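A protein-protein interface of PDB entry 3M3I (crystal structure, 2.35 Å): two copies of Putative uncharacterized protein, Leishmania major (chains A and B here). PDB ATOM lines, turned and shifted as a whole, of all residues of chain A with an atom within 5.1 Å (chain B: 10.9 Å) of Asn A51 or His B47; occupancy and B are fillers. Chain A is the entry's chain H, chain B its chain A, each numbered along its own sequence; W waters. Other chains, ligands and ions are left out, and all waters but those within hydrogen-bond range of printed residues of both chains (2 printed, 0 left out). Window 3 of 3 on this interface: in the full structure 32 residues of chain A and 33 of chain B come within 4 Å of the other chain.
NE2 of His B47 is in hydrogen-bond range of O of Asp A50, at 3.0 Å.
Val B49 touches its own counterpart, Val A49. Val A49 touches Asp B50, and with the chains exchanged Asp A50 touches Val B49. Positions printed for both chains: 49, 50, 51, 55, 57 and 180. Of the 8 pairs that touch across the chains among the printed residues, 3 have their exchanged pair printed and touching as well.
N of His B47 is in hydrogen-bond range of OG of Ser B45, at 3.0 Å. The backbone NH (N) of Ala B59 lies within hydrogen-bond range of the backbone carbonyl oxygen (O) of His B47, at 2.9 Å. OD1 of Asp B50 lies within salt-bridge range of NH1 of Arg B56 (3.6 Å). The side-chain hydroxyl (OG) of Ser B179 lies within hydrogen-bond range of the backbone carbonyl oxygen (O) of Ala B59 (2.9 Å). O of Ala B59 sits at hydrogen-bond distance from N of Gly B181 (3.5 Å). The side-chain hydroxyl (OG) of Ser A80 sits at hydrogen-bond distance from the backbone carbonyl oxygen (O) of Pro A180 (3.1 Å).
Among the printed residues, pairs that only touch across the chains: Val A49 with Val B49, Val A49 with Asp B50, Asp A50 with Val B49, Asn A51 with His B47, Glu A52 with His B47, Pro A180 with His B47 and Pro A180 with Ala B59.
Water W2 bridges OE2 of Glu A52 and OG of Ser B45. Water W1 lies within hydrogen-bond range of N of Asp A50 (3.2 Å) and N of Asp B50 (3.4 Å).
Hydrophobic or aromatic side chains of chain B within 4 Å of the printed part of chain A: His B47, Val B49 and Ala B59. Of the 12 printed residues of chain A, 5 touch a printed residue of chain B. Hydrophobic or aromatic side chains of chain A within 4 Å of the printed part of chain B: Val A49 and Pro A180.
Asn A51 touches just one residue of chain B: His B47. His B47 touches just these residues of chain A: Asp A50, Asn A51, Glu A52 and Pro A180. Of chain B, only His B47 comes within 4 Å of Glu A52. No residue of chain B comes within 4 Å of Glu A53. Gly A54 touches none of the printed residues of chain B. No residue of chain B comes within 4 Å of Asn A55. No residue of chain B comes within 4 Å of Arg A57. No residue of chain B comes within 4 Å of Cys A79. Of chain B, only His B47 and Ala B59 come within 4 Å of Pro A180. Of the printed residues of chain A, Val B49 touches Val A49 and Asp A50. Printed residues of chain A within 4 Å of Asp B50: Val A49. Of the printed residues of chain A, Ala B59 touches Pro A180 (3.7 Å). Asp A186 touches none of the printed residues of chain B. Asn B51 touches none of the printed residues of chain A. The nearest printed residue of chain A that does not touch His B47 is Glu A53 (5.8 Å). The nearest printed residue of chain B that does not touch Val A49 is Pro B180 (4.4 Å).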
ATOM      1  N   VAL A  49      25.983 -26.258 -15.308  1.00  0.00           N
ATOM      2  CA  VAL A  49      25.380 -26.725 -16.548  1.00  0.00           C
ATOM      3  C   VAL A  49      24.474 -27.913 -16.241  1.00  0.00           C
ATOM      4  O   VAL A  49      24.615 -28.545 -15.199  1.00  0.00           O
ATOM      5  CB  VAL A  49      26.478 -27.151 -17.574  1.00  0.00           C
ATOM      6  CG1 VAL A  49      27.400 -26.000 -17.897  1.00  0.00           C
ATOM      7  CG2 VAL A  49      27.294 -28.308 -17.050  1.00  0.00           C
ATOM      8  N   ASP A  50      23.529 -28.191 -17.131  1.00  0.00           N
ATOM      9  CA  ASP A  50      22.749 -29.425 -17.091  1.00  0.00           C
ATOM     10  C   ASP A  50      23.599 -30.528 -17.686  1.00  0.00           C
ATOM     11  O   ASP A  50      24.283 -30.299 -18.683  1.00  0.00           O
ATOM     12  CB  ASP A  50      21.466 -29.297 -17.921  1.00  0.00           C
ATOM     13  CG  ASP A  50      20.338 -28.606 -17.175  1.00  0.00           C
ATOM     14  OD1 ASP A  50      20.525 -28.265 -15.986  1.00  0.00           O
ATOM     15  OD2 ASP A  50      19.253 -28.423 -17.780  1.00  0.00           O
ATOM     16  N   ASN A  51      23.575 -31.709 -17.080  1.00  0.00           N
ATOM     17  CA  ASN A  51      24.336 -32.842 -17.606  1.00  0.00           C
ATOM     18  C   ASN A  51      23.477 -33.749 -18.483  1.00  0.00           C
ATOM     19  O   ASN A  51      22.367 -33.377 -18.837  1.00  0.00           O
ATOM     20  CB  ASN A  51      25.075 -33.594 -16.485  1.00  0.00           C
ATOM     21  CG  ASN A  51      24.194 -34.538 -15.708  1.00  0.00           C
ATOM     22  OD1 ASN A  51      22.961 -34.473 -15.772  1.00  0.00           O
ATOM     23  ND2 ASN A  51      24.828 -35.423 -14.947  1.00  0.00           N
ATOM     24  N   GLU A  52      23.988 -34.921 -18.838  1.00  0.00           N
ATOM     25  CA  GLU A  52      23.302 -35.810 -19.789  1.00  0.00           C
ATOM     26  C   GLU A  52      21.990 -36.407 -19.252  1.00  0.00           C
ATOM     27  O   GLU A  52      21.190 -36.945 -20.024  1.00  0.00           O
ATOM     28  CB  GLU A  52      24.243 -36.942 -20.247  1.00  0.00           C
ATOM     29  CG  GLU A  52      25.468 -36.493 -21.079  1.00  0.00           C
ATOM     30  CD  GLU A  52      26.664 -36.093 -20.230  1.00  0.00           C
ATOM     31  OE1 GLU A  52      26.476 -35.586 -19.102  1.00  0.00           O
ATOM     32  OE2 GLU A  52      27.811 -36.274 -20.694  1.00  0.00           O
ATOM     33  N   GLU A  53      21.779 -36.322 -17.932  1.00  0.00           N
ATOM     34  CA  GLU A  53      20.542 -36.792 -17.288  1.00  0.00           C
ATOM     35  C   GLU A  53      19.605 -35.657 -16.818  1.00  0.00           C
ATOM     36  O   GLU A  53      18.544 -35.930 -16.255  1.00  0.00           O
ATOM     37  CB  GLU A  53      20.888 -37.733 -16.138  1.00  0.00           C
ATOM     38  CG  GLU A  53      21.404 -39.100 -16.630  1.00  0.00           C
ATOM     39  CD  GLU A  53      22.400 -39.779 -15.682  1.00  0.00           C
ATOM     40  OE1 GLU A  53      22.908 -39.128 -14.742  1.00  0.00           O
ATOM     41  OE2 GLU A  53      22.685 -40.980 -15.894  1.00  0.00           O
ATOM     42  N   GLY A  54      19.973 -34.400 -17.087  1.00  0.00           N
ATOM     43  CA  GLY A  54      19.157 -33.253 -16.695  1.00  0.00           C
ATOM     44  C   GLY A  54      19.423 -32.695 -15.295  1.00  0.00           C
ATOM     45  O   GLY A  54      18.717 -31.791 -14.845  1.00  0.00           O
ATOM     46  N   ASN A  55      20.447 -33.216 -14.615  1.00  0.00           N
ATOM     47  CA  ASN A  55      20.837 -32.750 -13.290  1.00  0.00           C
ATOM     48  C   ASN A  55      21.822 -31.586 -13.361  1.00  0.00           C
ATOM     49  O   ASN A  55      22.600 -31.488 -14.309  1.00  0.00           O
ATOM     50  CB  ASN A  55      21.457 -33.901 -12.512  1.00  0.00           C
ATOM     51  CG  ASN A  55      20.439 -34.961 -12.127  1.00  0.00           C
ATOM     52  OD1 ASN A  55      19.368 -34.648 -11.600  1.00  0.00           O
ATOM     53  ND2 ASN A  55      20.781 -36.229 -12.368  1.00  0.00           N
ATOM     54  N   ARG A  57      25.119 -29.698 -12.664  1.00  0.00           N
ATOM     55  CA  ARG A  57      26.488 -30.041 -12.335  1.00  0.00           C
ATOM     56  C   ARG A  57      27.374 -28.846 -12.611  1.00  0.00           C
ATOM     57  O   ARG A  57      26.968 -27.941 -13.316  1.00  0.00           O
ATOM     58  CB  ARG A  57      26.926 -31.253 -13.155  1.00  0.00           C
ATOM     59  CG  ARG A  57      26.161 -32.546 -12.816  1.00  0.00           C
ATOM     60  CD  ARG A  57      26.591 -33.125 -11.475  1.00  0.00           C
ATOM     61  NE  ARG A  57      25.867 -34.340 -11.119  1.00  0.00           N
ATOM     62  CZ  ARG A  57      24.711 -34.377 -10.440  1.00  0.00           C
ATOM     63  NH1 ARG A  57      24.102 -33.263 -10.023  1.00  0.00           N
ATOM     64  NH2 ARG A  57      24.144 -35.550 -10.191  1.00  0.00           N
ATOM     65  N   CYS A  79      28.284 -40.842 -15.986  1.00  0.00           N
ATOM     66  CA  CYS A  79      27.370 -40.501 -17.086  1.00  0.00           C
ATOM     67  C   CYS A  79      27.878 -39.319 -17.923  1.00  0.00           C
ATOM     68  O   CYS A  79      27.197 -38.880 -18.832  1.00  0.00           O
ATOM     69  CB  CYS A  79      25.935 -40.266 -16.572  1.00  0.00           C
ATOM     70  SG  CYS A  79      25.468 -38.572 -16.191  1.00  0.00           S
ATOM     71  N   SER A  80      29.084 -38.833 -17.617  1.00  0.00           N
ATOM     72  CA  SER A  80      29.761 -37.793 -18.389  1.00  0.00           C
ATOM     73  C   SER A  80      31.106 -38.310 -18.862  1.00  0.00           C
ATOM     74  O   SER A  80      31.644 -39.249 -18.296  1.00  0.00           O
ATOM     75  CB  SER A  80      30.021 -36.547 -17.539  1.00  0.00           C
ATOM     76  OG  SER A  80      28.854 -35.788 -17.356  1.00  0.00           O
ATOM     77  N   PRO A 180      30.391 -32.785 -18.366  1.00  0.00           N
ATOM     78  CA  PRO A 180      29.946 -32.079 -17.175  1.00  0.00           C
ATOM     79  C   PRO A 180      30.426 -32.719 -15.873  1.00  0.00           C
ATOM     80  O   PRO A 180      30.834 -33.894 -15.856  1.00  0.00           O
ATOM     81  CB  PRO A 180      28.419 -32.133 -17.286  1.00  0.00           C
ATOM     82  CG  PRO A 180      28.175 -32.192 -18.740  1.00  0.00           C
ATOM     83  CD  PRO A 180      29.256 -33.063 -19.266  1.00  0.00           C
ATOM     84  N   ASP A 186      26.569 -39.871  -9.394  1.00  0.00           N
ATOM     85  CA  ASP A 186      26.638 -40.406 -10.772  1.00  0.00           C
ATOM     86  C   ASP A 186      27.704 -41.503 -10.936  1.00  0.00           C
ATOM     87  O   ASP A 186      27.741 -42.215 -11.958  1.00  0.00           O
ATOM     88  CB  ASP A 186      26.943 -39.299 -11.775  1.00  0.00           C
ATOM     89  CG  ASP A 186      26.008 -38.101 -11.646  1.00  0.00           C
ATOM     90  OD1 ASP A 186      24.798 -38.300 -11.421  1.00  0.00           O
ATOM     91  OD2 ASP A 186      26.496 -36.951 -11.788  1.00  0.00           O
ATOM     92  N   VAL B  43      39.262 -33.960 -28.950  1.00  0.00           N
ATOM     93  CA  VAL B  43      37.864 -34.313 -28.766  1.00  0.00           C
ATOM     94  C   VAL B  43      36.994 -33.120 -28.442  1.00  0.00           C
ATOM     95  O   VAL B  43      37.458 -32.102 -27.935  1.00  0.00           O
ATOM     96  CB  VAL B  43      37.659 -35.393 -27.685  1.00  0.00           C
ATOM     97  CG1 VAL B  43      38.543 -36.601 -27.982  1.00  0.00           C
ATOM     98  CG2 VAL B  43      37.934 -34.833 -26.303  1.00  0.00           C
ATOM     99  N   ARG B  44      35.716 -33.307 -28.750  1.00  0.00           N
ATOM    100  CA  ARG B  44      34.652 -32.356 -28.508  1.00  0.00           C
ATOM    101  C   ARG B  44      33.434 -33.129 -27.945  1.00  0.00           C
ATOM    102  O   ARG B  44      32.879 -33.989 -28.619  1.00  0.00           O
ATOM    103  CB  ARG B  44      34.309 -31.653 -29.835  1.00  0.00           C
ATOM    104  CG  ARG B  44      35.125 -30.372 -30.078  1.00  0.00           C
ATOM    105  CD  ARG B  44      35.624 -30.184 -31.508  1.00  0.00           C
ATOM    106  NE  ARG B  44      34.555 -29.872 -32.458  1.00  0.00           N
ATOM    107  CZ  ARG B  44      33.945 -28.690 -32.572  1.00  0.00           C
ATOM    108  NH1 ARG B  44      34.265 -27.670 -31.772  1.00  0.00           N
ATOM    109  NH2 ARG B  44      32.991 -28.532 -33.490  1.00  0.00           N
ATOM    110  N   SER B  45      33.044 -32.838 -26.710  1.00  0.00           N
ATOM    111  CA  SER B  45      31.848 -33.441 -26.092  1.00  0.00           C
ATOM    112  C   SER B  45      30.660 -33.592 -27.043  1.00  0.00           C
ATOM    113  O   SER B  45      30.330 -32.683 -27.793  1.00  0.00           O
ATOM    114  CB  SER B  45      31.392 -32.602 -24.882  1.00  0.00           C
ATOM    115  OG  SER B  45      30.217 -33.152 -24.262  1.00  0.00           O
ATOM    116  N   ALA B  46      30.007 -34.747 -26.983  1.00  0.00           N
ATOM    117  CA  ALA B  46      28.760 -34.970 -27.707  1.00  0.00           C
ATOM    118  C   ALA B  46      27.630 -34.095 -27.152  1.00  0.00           C
ATOM    119  O   ALA B  46      26.716 -33.726 -27.885  1.00  0.00           O
ATOM    120  CB  ALA B  46      28.372 -36.435 -27.628  1.00  0.00           C
ATOM    121  N   HIS B  47      27.714 -33.769 -25.859  1.00  0.00           N
ATOM    122  CA  HIS B  47      26.650 -33.099 -25.106  1.00  0.00           C
ATOM    123  C   HIS B  47      26.874 -31.585 -25.093  1.00  0.00           C
ATOM    124  O   HIS B  47      27.968 -31.117 -24.786  1.00  0.00           O
ATOM    125  CB  HIS B  47      26.639 -33.654 -23.678  1.00  0.00           C
ATOM    126  CG  HIS B  47      25.670 -32.981 -22.749  1.00  0.00           C
ATOM    127  ND1 HIS B  47      24.322 -33.262 -22.743  1.00  0.00           N
ATOM    128  CD2 HIS B  47      25.868 -32.079 -21.757  1.00  0.00           C
ATOM    129  CE1 HIS B  47      23.728 -32.545 -21.808  1.00  0.00           C
ATOM    130  NE2 HIS B  47      24.644 -31.821 -21.191  1.00  0.00           N
ATOM    131  N   LYS B  48      25.829 -30.834 -25.429  1.00  0.00           N
ATOM    132  CA  LYS B  48      25.881 -29.378 -25.485  1.00  0.00           C
ATOM    133  C   LYS B  48      25.298 -28.729 -24.222  1.00  0.00           C
ATOM    134  O   LYS B  48      24.373 -29.256 -23.609  1.00  0.00           O
ATOM    135  CB  LYS B  48      25.101 -28.875 -26.704  1.00  0.00           C
ATOM    136  CG  LYS B  48      25.741 -29.187 -28.051  1.00  0.00           C
ATOM    137  CD  LYS B  48      25.369 -28.114 -29.079  1.00  0.00           C
ATOM    138  CE  LYS B  48      26.195 -28.189 -30.375  1.00  0.00           C
ATOM    139  NZ  LYS B  48      25.414 -28.621 -31.591  1.00  0.00           N
ATOM    140  N   VAL B  49      25.839 -27.568 -23.862  1.00  0.00           N
ATOM    141  CA  VAL B  49      25.429 -26.857 -22.659  1.00  0.00           C
ATOM    142  C   VAL B  49      25.356 -25.370 -22.980  1.00  0.00           C
ATOM    143  O   VAL B  49      25.819 -24.941 -24.038  1.00  0.00           O
ATOM    144  CB  VAL B  49      26.427 -27.109 -21.467  1.00  0.00           C
ATOM    145  CG1 VAL B  49      26.570 -28.564 -21.213  1.00  0.00           C
ATOM    146  CG2 VAL B  49      27.817 -26.519 -21.750  1.00  0.00           C
ATOM    147  N   ASP B  50      24.771 -24.600 -22.066  1.00  0.00           N
ATOM    148  CA  ASP B  50      24.789 -23.144 -22.125  1.00  0.00           C
ATOM    149  C   ASP B  50      26.035 -22.613 -21.412  1.00  0.00           C
ATOM    150  O   ASP B  50      26.323 -22.979 -20.255  1.00  0.00           O
ATOM    151  CB  ASP B  50      23.531 -22.561 -21.464  1.00  0.00           C
ATOM    152  CG  ASP B  50      22.266 -22.708 -22.331  1.00  0.00           C
ATOM    153  OD1 ASP B  50      22.332 -22.583 -23.581  1.00  0.00           O
ATOM    154  OD2 ASP B  50      21.184 -22.909 -21.752  1.00  0.00           O
ATOM    155  N   ASN B  51      26.784 -21.756 -22.095  1.00  0.00           N
ATOM    156  CA  ASN B  51      27.984 -21.175 -21.508  1.00  0.00           C
ATOM    157  C   ASN B  51      27.685 -19.964 -20.581  1.00  0.00           C
ATOM    158  O   ASN B  51      26.535 -19.655 -20.289  1.00  0.00           O
ATOM    159  CB  ASN B  51      28.975 -20.802 -22.625  1.00  0.00           C
ATOM    160  CG  ASN B  51      28.495 -19.645 -23.434  1.00  0.00           C
ATOM    161  OD1 ASN B  51      27.389 -19.146 -23.196  1.00  0.00           O
ATOM    162  ND2 ASN B  51      29.307 -19.186 -24.387  1.00  0.00           N
ATOM    163  N   ASN B  55      25.068 -18.907 -24.615  1.00  0.00           N
ATOM    164  CA  ASN B  55      25.211 -19.583 -25.899  1.00  0.00           C
ATOM    165  C   ASN B  55      25.430 -21.094 -25.801  1.00  0.00           C
ATOM    166  O   ASN B  55      26.078 -21.577 -24.877  1.00  0.00           O
ATOM    167  CB  ASN B  55      26.385 -18.968 -26.653  1.00  0.00           C
ATOM    168  CG  ASN B  55      26.245 -17.462 -26.835  1.00  0.00           C
ATOM    169  OD1 ASN B  55      25.163 -16.960 -27.133  1.00  0.00           O
ATOM    170  ND2 ASN B  55      27.347 -16.743 -26.679  1.00  0.00           N
ATOM    171  N   ARG B  56      24.913 -21.826 -26.779  1.00  0.00           N
ATOM    172  CA  ARG B  56      25.100 -23.276 -26.847  1.00  0.00           C
ATOM    173  C   ARG B  56      26.511 -23.627 -27.282  1.00  0.00           C
ATOM    174  O   ARG B  56      26.988 -23.184 -28.339  1.00  0.00           O
ATOM    175  CB  ARG B  56      24.098 -23.930 -27.802  1.00  0.00           C
ATOM    176  CG  ARG B  56      22.645 -23.683 -27.433  1.00  0.00           C
ATOM    177  CD  ARG B  56      22.261 -24.312 -26.108  1.00  0.00           C
ATOM    178  NE  ARG B  56      22.105 -25.759 -26.214  1.00  0.00           N
ATOM    179  CZ  ARG B  56      21.795 -26.552 -25.195  1.00  0.00           C
ATOM    180  NH1 ARG B  56      21.620 -26.044 -23.993  1.00  0.00           N
ATOM    181  NH2 ARG B  56      21.673 -27.858 -25.378  1.00  0.00           N
ATOM    182  N   ARG B  57      27.171 -24.421 -26.443  1.00  0.00           N
ATOM    183  CA  ARG B  57      28.548 -24.849 -26.651  1.00  0.00           C
ATOM    184  C   ARG B  57      28.648 -26.308 -26.256  1.00  0.00           C
ATOM    185  O   ARG B  57      27.780 -26.823 -25.547  1.00  0.00           O
ATOM    186  CB  ARG B  57      29.473 -24.026 -25.788  1.00  0.00           C
ATOM    187  CG  ARG B  57      29.474 -22.539 -26.100  1.00  0.00           C
ATOM    188  CD  ARG B  57      30.342 -22.204 -27.298  1.00  0.00           C
ATOM    189  NE  ARG B  57      30.280 -20.775 -27.613  1.00  0.00           N
ATOM    190  CZ  ARG B  57      29.365 -20.211 -28.407  1.00  0.00           C
ATOM    191  NH1 ARG B  57      28.424 -20.946 -28.988  1.00  0.00           N
ATOM    192  NH2 ARG B  57      29.393 -18.895 -28.616  1.00  0.00           N
ATOM    193  N   HIS B  58      29.676 -26.987 -26.738  1.00  0.00           N
ATOM    194  CA  HIS B  58      30.002 -28.319 -26.248  1.00  0.00           C
ATOM    195  C   HIS B  58      30.355 -28.229 -24.756  1.00  0.00           C
ATOM    196  O   HIS B  58      30.930 -27.229 -24.322  1.00  0.00           O
ATOM    197  CB  HIS B  58      31.193 -28.904 -27.028  1.00  0.00           C
ATOM    198  CG  HIS B  58      30.917 -29.105 -28.488  1.00  0.00           C
ATOM    199  ND1 HIS B  58      31.282 -28.188 -29.451  1.00  0.00           N
ATOM    200  CD2 HIS B  58      30.283 -30.107 -29.142  1.00  0.00           C
ATOM    201  CE1 HIS B  58      30.891 -28.630 -30.636  1.00  0.00           C
ATOM    202  NE2 HIS B  58      30.283 -29.793 -30.474  1.00  0.00           N
ATOM    203  N   ALA B  59      29.999 -29.253 -23.979  1.00  0.00           N
ATOM    204  CA  ALA B  59      30.374 -29.298 -22.569  1.00  0.00           C
ATOM    205  C   ALA B  59      31.840 -28.919 -22.412  1.00  0.00           C
ATOM    206  O   ALA B  59      32.177 -28.033 -21.637  1.00  0.00           O
ATOM    207  CB  ALA B  59      30.124 -30.677 -21.968  1.00  0.00           C
ATOM    208  N   TYR B  60      32.694 -29.614 -23.159  1.00  0.00           N
ATOM    209  CA  TYR B  60      34.120 -29.332 -23.204  1.00  0.00           C
ATOM    210  C   TYR B  60      34.651 -29.562 -24.612  1.00  0.00           C
ATOM    211  O   TYR B  60      34.028 -30.236 -25.422  1.00  0.00           O
ATOM    212  CB  TYR B  60      34.879 -30.225 -22.230  1.00  0.00           C
ATOM    213  CG  TYR B  60      34.877 -31.681 -22.635  1.00  0.00           C
ATOM    214  CD1 TYR B  60      35.912 -32.221 -23.371  1.00  0.00           C
ATOM    215  CD2 TYR B  60      33.826 -32.510 -22.296  1.00  0.00           C
ATOM    216  CE1 TYR B  60      35.895 -33.541 -23.755  1.00  0.00           C
ATOM    217  CE2 TYR B  60      33.808 -33.845 -22.681  1.00  0.00           C
ATOM    218  CZ  TYR B  60      34.846 -34.350 -23.415  1.00  0.00           C
ATOM    219  OH  TYR B  60      34.833 -35.669 -23.796  1.00  0.00           O
ATOM    220  N   THR B  61      35.811 -28.979 -24.874  1.00  0.00           N
ATOM    221  CA  THR B  61      36.595 -29.214 -26.065  1.00  0.00           C
ATOM    222  C   THR B  61      38.018 -29.319 -25.562  1.00  0.00           C
ATOM    223  O   THR B  61      38.363 -28.669 -24.587  1.00  0.00           O
ATOM    224  CB  THR B  61      36.464 -28.057 -27.080  1.00  0.00           C
ATOM    225  OG1 THR B  61      36.824 -26.825 -26.464  1.00  0.00           O
ATOM    226  CG2 THR B  61      35.033 -27.935 -27.613  1.00  0.00           C
ATOM    227  N   VAL B 178      39.011 -26.498 -22.656  1.00  0.00           N
ATOM    228  CA  VAL B 178      38.121 -25.372 -22.400  1.00  0.00           C
ATOM    229  C   VAL B 178      36.735 -25.916 -22.096  1.00  0.00           C
ATOM    230  O   VAL B 178      36.242 -26.765 -22.823  1.00  0.00           O
ATOM    231  CB  VAL B 178      38.070 -24.387 -23.586  1.00  0.00           C
ATOM    232  CG1 VAL B 178      37.344 -23.111 -23.176  1.00  0.00           C
ATOM    233  CG2 VAL B 178      39.469 -24.068 -24.081  1.00  0.00           C
ATOM    234  N   SER B 179      36.142 -25.469 -20.989  1.00  0.00           N
ATOM    235  CA  SER B 179      34.803 -25.917 -20.565  1.00  0.00           C
ATOM    236  C   SER B 179      34.045 -24.852 -19.770  1.00  0.00           C
ATOM    237  O   SER B 179      34.531 -24.390 -18.727  1.00  0.00           O
ATOM    238  CB  SER B 179      34.879 -27.178 -19.715  1.00  0.00           C
ATOM    239  OG  SER B 179      33.611 -27.484 -19.154  1.00  0.00           O
ATOM    240  N   PRO B 180      32.842 -24.468 -20.251  1.00  0.00           N
ATOM    241  CA  PRO B 180      32.199 -24.920 -21.483  1.00  0.00           C
ATOM    242  C   PRO B 180      33.043 -24.628 -22.738  1.00  0.00           C
ATOM    243  O   PRO B 180      33.889 -23.744 -22.724  1.00  0.00           O
ATOM    244  CB  PRO B 180      30.870 -24.146 -21.481  1.00  0.00           C
ATOM    245  CG  PRO B 180      30.600 -23.887 -20.065  1.00  0.00           C
ATOM    246  CD  PRO B 180      31.937 -23.601 -19.468  1.00  0.00           C
ATOM    247  N   GLY B 181      32.790 -25.371 -23.812  1.00  0.00           N
ATOM    248  CA  GLY B 181      33.762 -25.579 -24.886  1.00  0.00           C
ATOM    249  C   GLY B 181      34.218 -24.364 -25.669  1.00  0.00           C
ATOM    250  O   GLY B 181      33.573 -23.310 -25.657  1.00  0.00           O
ATOM    251  N   PHE B 182      35.335 -24.532 -26.369  1.00  0.00           N
ATOM    252  CA  PHE B 182      35.879 -23.490 -27.224  1.00  0.00           C
ATOM    253  C   PHE B 182      35.041 -23.277 -28.508  1.00  0.00           C
ATOM    254  O   PHE B 182      34.529 -24.223 -29.119  1.00  0.00           O
ATOM    255  CB  PHE B 182      37.342 -23.826 -27.577  1.00  0.00           C
ATOM    256  CG  PHE B 182      38.015 -22.781 -28.404  1.00  0.00           C
ATOM    257  CD1 PHE B 182      38.654 -21.719 -27.814  1.00  0.00           C
ATOM    258  CD2 PHE B 182      38.005 -22.856 -29.772  1.00  0.00           C
ATOM    259  CE1 PHE B 182      39.264 -20.753 -28.576  1.00  0.00           C
ATOM    260  CE2 PHE B 182      38.611 -21.889 -30.527  1.00  0.00           C
ATOM    261  CZ  PHE B 182      39.235 -20.840 -29.924  1.00  0.00           C
HETATM  262  O   HOH W   1      23.028 -26.054 -19.470  1.00  0.00           O
HETATM  263  O   HOH W   2      30.279 -35.164 -21.582  1.00  0.00           O
